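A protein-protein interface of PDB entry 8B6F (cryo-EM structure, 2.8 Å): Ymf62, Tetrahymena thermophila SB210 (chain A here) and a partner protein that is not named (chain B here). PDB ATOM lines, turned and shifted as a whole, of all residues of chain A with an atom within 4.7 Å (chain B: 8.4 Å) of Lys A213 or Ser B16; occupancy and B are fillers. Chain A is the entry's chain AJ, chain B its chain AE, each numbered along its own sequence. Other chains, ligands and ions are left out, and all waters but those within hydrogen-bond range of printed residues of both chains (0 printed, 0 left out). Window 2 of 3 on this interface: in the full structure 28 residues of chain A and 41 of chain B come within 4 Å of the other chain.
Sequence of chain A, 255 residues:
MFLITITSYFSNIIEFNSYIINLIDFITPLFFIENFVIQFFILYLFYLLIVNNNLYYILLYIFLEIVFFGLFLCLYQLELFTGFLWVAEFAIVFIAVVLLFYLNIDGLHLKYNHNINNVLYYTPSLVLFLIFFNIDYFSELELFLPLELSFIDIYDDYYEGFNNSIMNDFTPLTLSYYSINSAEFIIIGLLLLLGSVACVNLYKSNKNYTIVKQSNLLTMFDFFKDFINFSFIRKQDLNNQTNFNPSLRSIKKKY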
ATOM      1  N   THR A 210     -26.058 -20.168   6.736  1.00  0.00           N
ATOM      2  CA  THR A 210     -26.175 -18.716   6.793  1.00  0.00           C
ATOM      3  C   THR A 210     -25.135 -18.018   5.926  1.00  0.00           C
ATOM      4  O   THR A 210     -25.325 -16.851   5.573  1.00  0.00           O
ATOM      5  CB  THR A 210     -26.070 -18.217   8.238  1.00  0.00           C
ATOM      6  OG1 THR A 210     -26.075 -16.783   8.255  1.00  0.00           O
ATOM      7  CG2 THR A 210     -24.808 -18.719   8.915  1.00  0.00           C
ATOM      8  N   ILE A 211     -24.049 -18.706   5.568  1.00  0.00           N
ATOM      9  CA  ILE A 211     -23.024 -18.109   4.718  1.00  0.00           C
ATOM     10  C   ILE A 211     -23.396 -18.153   3.241  1.00  0.00           C
ATOM     11  O   ILE A 211     -22.835 -17.387   2.449  1.00  0.00           O
ATOM     12  CB  ILE A 211     -21.674 -18.821   4.925  1.00  0.00           C
ATOM     13  CG1 ILE A 211     -21.258 -18.769   6.397  1.00  0.00           C
ATOM     14  CG2 ILE A 211     -20.591 -18.201   4.047  1.00  0.00           C
ATOM     15  CD1 ILE A 211     -20.038 -19.613   6.726  1.00  0.00           C
ATOM     16  N   VAL A 212     -24.335 -19.016   2.848  1.00  0.00           N
ATOM     17  CA  VAL A 212     -24.609 -19.236   1.429  1.00  0.00           C
ATOM     18  C   VAL A 212     -24.911 -17.921   0.719  1.00  0.00           C
ATOM     19  O   VAL A 212     -24.349 -17.626  -0.342  1.00  0.00           O
ATOM     20  CB  VAL A 212     -25.767 -20.237   1.256  1.00  0.00           C
ATOM     21  CG1 VAL A 212     -26.164 -20.366  -0.207  1.00  0.00           C
ATOM     22  CG2 VAL A 212     -25.395 -21.585   1.828  1.00  0.00           C
ATOM     23  N   LYS A 213     -25.804 -17.113   1.285  1.00  0.00           N
ATOM     24  CA  LYS A 213     -26.341 -15.957   0.579  1.00  0.00           C
ATOM     25  C   LYS A 213     -25.641 -14.649   0.924  1.00  0.00           C
ATOM     26  O   LYS A 213     -26.027 -13.604   0.394  1.00  0.00           O
ATOM     27  CB  LYS A 213     -27.839 -15.822   0.862  1.00  0.00           C
ATOM     28  CG  LYS A 213     -28.675 -16.909   0.208  1.00  0.00           C
ATOM     29  CD  LYS A 213     -30.157 -16.627   0.336  1.00  0.00           C
ATOM     30  CE  LYS A 213     -30.974 -17.652  -0.433  1.00  0.00           C
ATOM     31  NZ  LYS A 213     -32.437 -17.389  -0.326  1.00  0.00           N
ATOM     32  N   GLN A 214     -24.631 -14.672   1.794  1.00  0.00           N
ATOM     33  CA  GLN A 214     -23.968 -13.428   2.173  1.00  0.00           C
ATOM     34  C   GLN A 214     -23.264 -12.793   0.981  1.00  0.00           C
ATOM     35  O   GLN A 214     -23.235 -11.565   0.849  1.00  0.00           O
ATOM     36  CB  GLN A 214     -22.977 -13.684   3.306  1.00  0.00           C
ATOM     37  CG  GLN A 214     -23.609 -14.306   4.531  1.00  0.00           C
ATOM     38  CD  GLN A 214     -22.645 -14.403   5.691  1.00  0.00           C
ATOM     39  OE1 GLN A 214     -21.539 -13.870   5.637  1.00  0.00           O
ATOM     40  NE2 GLN A 214     -23.060 -15.087   6.750  1.00  0.00           N
ATOM     41  N   SER A 215     -22.689 -13.614   0.102  1.00  0.00           N
ATOM     42  CA  SER A 215     -22.004 -13.085  -1.073  1.00  0.00           C
ATOM     43  C   SER A 215     -22.946 -12.256  -1.933  1.00  0.00           C
ATOM     44  O   SER A 215     -22.635 -11.115  -2.294  1.00  0.00           O
ATOM     45  CB  SER A 215     -21.409 -14.233  -1.888  1.00  0.00           C
ATOM     46  OG  SER A 215     -20.843 -13.751  -3.095  1.00  0.00           O
ATOM     47  N   ASN A 216     -24.105 -12.815  -2.281  1.00  0.00           N
ATOM     48  CA  ASN A 216     -25.057 -12.076  -3.101  1.00  0.00           C
ATOM     49  C   ASN A 216     -25.593 -10.857  -2.363  1.00  0.00           C
ATOM     50  O   ASN A 216     -25.792  -9.799  -2.967  1.00  0.00           O
ATOM     51  CB  ASN A 216     -26.204 -12.987  -3.531  1.00  0.00           C
ATOM     52  CG  ASN A 216     -27.159 -12.300  -4.486  1.00  0.00           C
ATOM     53  OD1 ASN A 216     -28.171 -11.736  -4.072  1.00  0.00           O
ATOM     54  ND2 ASN A 216     -26.833 -12.334  -5.772  1.00  0.00           N
ATOM     55  N   LEU A 217     -25.843 -10.989  -1.059  1.00  0.00           N
ATOM     56  CA  LEU A 217     -26.311  -9.848  -0.281  1.00  0.00           C
ATOM     57  C   LEU A 217     -25.339  -8.682  -0.394  1.00  0.00           C
ATOM     58  O   LEU A 217     -25.734  -7.555  -0.713  1.00  0.00           O
ATOM     59  CB  LEU A 217     -26.496 -10.254   1.182  1.00  0.00           C
ATOM     60  CG  LEU A 217     -26.958  -9.153   2.140  1.00  0.00           C
ATOM     61  CD1 LEU A 217     -28.367  -8.704   1.803  1.00  0.00           C
ATOM     62  CD2 LEU A 217     -26.878  -9.626   3.577  1.00  0.00           C
ATOM     63  N   TRP B   9     -20.611 -12.838  12.879  1.00  0.00           N
ATOM     64  CA  TRP B   9     -21.699 -12.003  12.392  1.00  0.00           C
ATOM     65  C   TRP B   9     -22.681 -12.848  11.593  1.00  0.00           C
ATOM     66  O   TRP B   9     -22.305 -13.840  10.964  1.00  0.00           O
ATOM     67  CB  TRP B   9     -21.161 -10.835  11.546  1.00  0.00           C
ATOM     68  CG  TRP B   9     -21.123 -11.071  10.065  1.00  0.00           C
ATOM     69  CD1 TRP B   9     -20.562 -12.129   9.413  1.00  0.00           C
ATOM     70  CD2 TRP B   9     -21.649 -10.209   9.050  1.00  0.00           C
ATOM     71  NE1 TRP B   9     -20.716 -11.985   8.057  1.00  0.00           N
ATOM     72  CE2 TRP B   9     -21.382 -10.814   7.808  1.00  0.00           C
ATOM     73  CE3 TRP B   9     -22.329  -8.986   9.073  1.00  0.00           C
ATOM     74  CZ2 TRP B   9     -21.770 -10.240   6.600  1.00  0.00           C
ATOM     75  CZ3 TRP B   9     -22.713  -8.417   7.871  1.00  0.00           C
ATOM     76  CH2 TRP B   9     -22.432  -9.045   6.651  1.00  0.00           C
ATOM     77  N   LYS B  10     -23.950 -12.445  11.634  1.00  0.00           N
ATOM     78  CA  LYS B  10     -25.020 -13.137  10.917  1.00  0.00           C
ATOM     79  C   LYS B  10     -25.898 -12.097  10.229  1.00  0.00           C
ATOM     80  O   LYS B  10     -26.774 -11.499  10.872  1.00  0.00           O
ATOM     81  CB  LYS B  10     -25.850 -14.006  11.856  1.00  0.00           C
ATOM     82  CG  LYS B  10     -27.068 -14.628  11.191  1.00  0.00           C
ATOM     83  CD  LYS B  10     -27.796 -15.581  12.119  1.00  0.00           C
ATOM     84  CE  LYS B  10     -29.052 -16.126  11.456  1.00  0.00           C
ATOM     85  NZ  LYS B  10     -29.820 -17.031  12.353  1.00  0.00           N
ATOM     86  N   PRO B  11     -25.704 -11.858   8.937  1.00  0.00           N
ATOM     87  CA  PRO B  11     -26.540 -10.886   8.230  1.00  0.00           C
ATOM     88  C   PRO B  11     -27.914 -11.461   7.910  1.00  0.00           C
ATOM     89  O   PRO B  11     -28.171 -12.657   8.044  1.00  0.00           O
ATOM     90  CB  PRO B  11     -25.746 -10.604   6.952  1.00  0.00           C
ATOM     91  CG  PRO B  11     -25.019 -11.861   6.699  1.00  0.00           C
ATOM     92  CD  PRO B  11     -24.677 -12.435   8.049  1.00  0.00           C
ATOM     93  N   GLU B  12     -28.804 -10.570   7.482  1.00  0.00           N
ATOM     94  CA  GLU B  12     -30.167 -10.926   7.111  1.00  0.00           C
ATOM     95  C   GLU B  12     -30.371 -10.662   5.628  1.00  0.00           C
ATOM     96  O   GLU B  12     -30.137  -9.546   5.154  1.00  0.00           O
ATOM     97  CB  GLU B  12     -31.183 -10.138   7.938  1.00  0.00           C
ATOM     98  CG  GLU B  12     -32.626 -10.399   7.545  1.00  0.00           C
ATOM     99  CD  GLU B  12     -33.612  -9.843   8.550  1.00  0.00           C
ATOM    100  OE1 GLU B  12     -33.166  -9.352   9.608  1.00  0.00           O
ATOM    101  OE2 GLU B  12     -34.830  -9.900   8.286  1.00  0.00           O
ATOM    102  N   SER B  13     -30.813 -11.695   4.897  1.00  0.00           N
ATOM    103  CA  SER B  13     -31.082 -11.591   3.474  1.00  0.00           C
ATOM    104  C   SER B  13     -32.583 -11.496   3.222  1.00  0.00           C
ATOM    105  O   SER B  13     -33.381 -12.020   4.004  1.00  0.00           O
ATOM    106  CB  SER B  13     -30.516 -12.805   2.730  1.00  0.00           C
ATOM    107  OG  SER B  13     -30.787 -12.738   1.342  1.00  0.00           O
ATOM    108  N   PRO B  14     -33.011 -10.835   2.147  1.00  0.00           N
ATOM    109  CA  PRO B  14     -34.453 -10.693   1.902  1.00  0.00           C
ATOM    110  C   PRO B  14     -35.141 -12.044   1.777  1.00  0.00           C
ATOM    111  O   PRO B  14     -34.725 -12.903   0.995  1.00  0.00           O
ATOM    112  CB  PRO B  14     -34.515  -9.901   0.590  1.00  0.00           C
ATOM    113  CG  PRO B  14     -33.211  -9.204   0.499  1.00  0.00           C
ATOM    114  CD  PRO B  14     -32.213 -10.117   1.137  1.00  0.00           C
ATOM    115  N   ARG B  15     -36.202 -12.226   2.561  1.00  0.00           N
ATOM    116  CA  ARG B  15     -37.066 -13.401   2.456  1.00  0.00           C
ATOM    117  C   ARG B  15     -36.257 -14.694   2.532  1.00  0.00           C
ATOM    118  O   ARG B  15     -36.482 -15.639   1.773  1.00  0.00           O
ATOM    119  CB  ARG B  15     -37.888 -13.348   1.168  1.00  0.00           C
ATOM    120  CG  ARG B  15     -39.077 -14.289   1.156  1.00  0.00           C
ATOM    121  CD  ARG B  15     -39.689 -14.408  -0.228  1.00  0.00           C
ATOM    122  NE  ARG B  15     -40.307 -13.166  -0.680  1.00  0.00           N
ATOM    123  CZ  ARG B  15     -39.701 -12.236  -1.405  1.00  0.00           C
ATOM    124  NH1 ARG B  15     -38.436 -12.359  -1.773  1.00  0.00           N
ATOM    125  NH2 ARG B  15     -40.381 -11.156  -1.773  1.00  0.00           N
ATOM    126  N   SER B  16     -35.303 -14.738   3.458  1.00  0.00           N
ATOM    127  CA  SER B  16     -34.457 -15.905   3.670  1.00  0.00           C
ATOM    128  C   SER B  16     -34.612 -16.388   5.104  1.00  0.00           C
ATOM    129  O   SER B  16     -34.466 -15.604   6.045  1.00  0.00           O
ATOM    130  CB  SER B  16     -32.991 -15.577   3.380  1.00  0.00           C
ATOM    131  OG  SER B  16     -32.164 -16.707   3.591  1.00  0.00           O
ATOM    132  N   ASN B  17     -34.910 -17.679   5.267  1.00  0.00           N
ATOM    133  CA  ASN B  17     -35.097 -18.228   6.607  1.00  0.00           C
ATOM    134  C   ASN B  17     -33.774 -18.357   7.349  1.00  0.00           C
ATOM    135  O   ASN B  17     -33.682 -18.001   8.529  1.00  0.00           O
ATOM    136  CB  ASN B  17     -35.797 -19.583   6.529  1.00  0.00           C
ATOM    137  CG  ASN B  17     -37.241 -19.470   6.085  1.00  0.00           C
ATOM    138  OD1 ASN B  17     -37.623 -18.517   5.409  1.00  0.00           O
ATOM    139  ND2 ASN B  17     -38.056 -20.442   6.475  1.00  0.00           N
ATOM    140  N   VAL B  18     -32.739 -18.873   6.682  1.00  0.00           N
ATOM    141  CA  VAL B  18     -31.455 -19.072   7.350  1.00  0.00           C
ATOM    142  C   VAL B  18     -30.853 -17.734   7.757  1.00  0.00           C
ATOM    143  O   VAL B  18     -30.322 -17.587   8.865  1.00  0.00           O
ATOM    144  CB  VAL B  18     -30.500 -19.885   6.455  1.00  0.00           C
ATOM    145  CG1 VAL B  18     -31.083 -21.255   6.170  1.00  0.00           C
ATOM    146  CG2 VAL B  18     -30.209 -19.154   5.151  1.00  0.00           C
ATOM    147  N   ASN B  19     -30.916 -16.741   6.872  1.00  0.00           N
ATOM    148  CA  ASN B  19     -30.435 -15.394   7.176  1.00  0.00           C
ATOM    149  C   ASN B  19     -31.585 -14.573   7.760  1.00  0.00           C
ATOM    150  O   ASN B  19     -32.138 -13.669   7.135  1.00  0.00           O
ATOM    151  CB  ASN B  19     -29.857 -14.737   5.929  1.00  0.00           C
ATOM    152  CG  ASN B  19     -28.632 -15.454   5.407  1.00  0.00           C
ATOM    153  OD1 ASN B  19     -28.725 -16.303   4.524  1.00  0.00           O
ATOM    154  ND2 ASN B  19     -27.472 -15.115   5.955  1.00  0.00           N
ATOM    155  N   SER B  20     -31.948 -14.918   8.991  1.00  0.00           N
ATOM    156  CA  SER B  20     -33.068 -14.271   9.662  1.00  0.00           C
ATOM    157  C   SER B  20     -33.031 -14.645  11.134  1.00  0.00           C
ATOM    158  O   SER B  20     -32.249 -15.499  11.560  1.00  0.00           O
ATOM    159  CB  SER B  20     -34.402 -14.678   9.029  1.00  0.00           C
ATOM    160  OG  SER B  20     -35.497 -14.171   9.769  1.00  0.00           O
ATOM    161  N   LYS B  21     -33.889 -13.989  11.912  1.00  0.00           N
ATOM    162  CA  LYS B  21     -34.035 -14.317  13.323  1.00  0.00           C
ATOM    163  C   LYS B  21     -34.792 -15.627  13.474  1.00  0.00           C
ATOM    164  O   LYS B  21     -36.027 -15.642  13.478  1.00  0.00           O
ATOM    165  CB  LYS B  21     -34.764 -13.200  14.073  1.00  0.00           C
ATOM    166  CG  LYS B  21     -34.048 -11.862  14.064  1.00  0.00           C
ATOM    167  CD  LYS B  21     -32.715 -11.934  14.785  1.00  0.00           C
ATOM    168  CE  LYS B  21     -32.070 -10.563  14.877  1.00  0.00           C
ATOM    169  NZ  LYS B  21     -30.722 -10.636  15.497  1.00  0.00           N
ATOM    170  N   GLN B  22     -34.065 -16.732  13.591  1.00  0.00           N
ATOM    171  CA  GLN B  22     -34.675 -18.042  13.758  1.00  0.00           C
ATOM    172  C   GLN B  22     -35.057 -18.332  15.202  1.00  0.00           C
ATOM    173  O   GLN B  22     -35.407 -19.473  15.520  1.00  0.00           O
ATOM    174  CB  GLN B  22     -33.727 -19.126  13.240  1.00  0.00           C
ATOM    175  CG  GLN B  22     -33.516 -19.081  11.736  1.00  0.00           C
ATOM    176  CD  GLN B  22     -32.413 -20.010  11.279  1.00  0.00           C
ATOM    177  OE1 GLN B  22     -31.349 -20.073  11.890  1.00  0.00           O
ATOM    178  NE2 GLN B  22     -32.666 -20.746  10.205  1.00  0.00           N
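The side-chain amino group (NZ) of Lys B10 is in hydrogen-bond range of the backbone carbonyl oxygen (O) of Ser B20.
NZ of Lys B10 is in hydrogen-bond range of OE1 of Gln B22, 3.4 Å away.
O of Pro B11 sits at hydrogen-bond distance from ND2 of Asn B19 (3.3 Å).
N of Ser B13 is in hydrogen-bond range of O of Asn B19.
The backbone carbonyl oxygen (O) of Thr A210 sits at hydrogen-bond distance from the side-chain amide nitrogen (NE2) of Gln A214.
The indole nitrogen (NE1) of Trp B9 is in hydrogen-bond range of the side-chain amide oxygen (OE1) of Gln A214 (3.2 Å).
O of Thr A210 is in hydrogen-bond range of ND2 of Asn B19 (2.8 Å).
Among the printed residues, merely in contact across the chains: Thr A210 with Lys B10 (3.8 Å), Lys A213 with Ser B16 (3.8 Å), Lys A213 with Asn B19 (3.8 Å), Gln A214 with Pro B11 (3.4 Å), Leu A217 with Pro B11 (3.7 Å) and Leu A217 with Glu B12 (3.6 Å).
Lys A213 touches just these residues of chain B: Ser B16 (3.8 Å) and Asn B19 (3.8 Å).
Of chain A, only Lys A213 (3.8 Å) comes within 4 Å of Ser B16.
Of the printed residues of chain B, Thr A210 touches Lys B10 (3.8 Å) and Asn B19 (2.8 Å).
Printed residues of chain B within 4 Å of Leu A217: Pro B11 and Glu B12.
Val A212 touches none of the printed residues of chain B.
Ser A215 touches none of the printed residues of chain B.
Printed residues of chain A that touch a printed residue of chain B: Thr A210, Lys A213, Gln A214 and Leu A217.
Hydrophobic or aromatic side chains of chain A within 4 Å of the printed part of chain B: Leu A217.
Of the 14 printed residues of chain B, 6 touch a printed residue of chain A.
Hydrophobic or aromatic side chains of chain B that line the printed part of chain A: Trp B9 and Pro B11.
Among the printed residues, no Asp or Glu carboxylate lies within 4 Å of a Lys or Arg side-chain nitrogen of the other chain.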
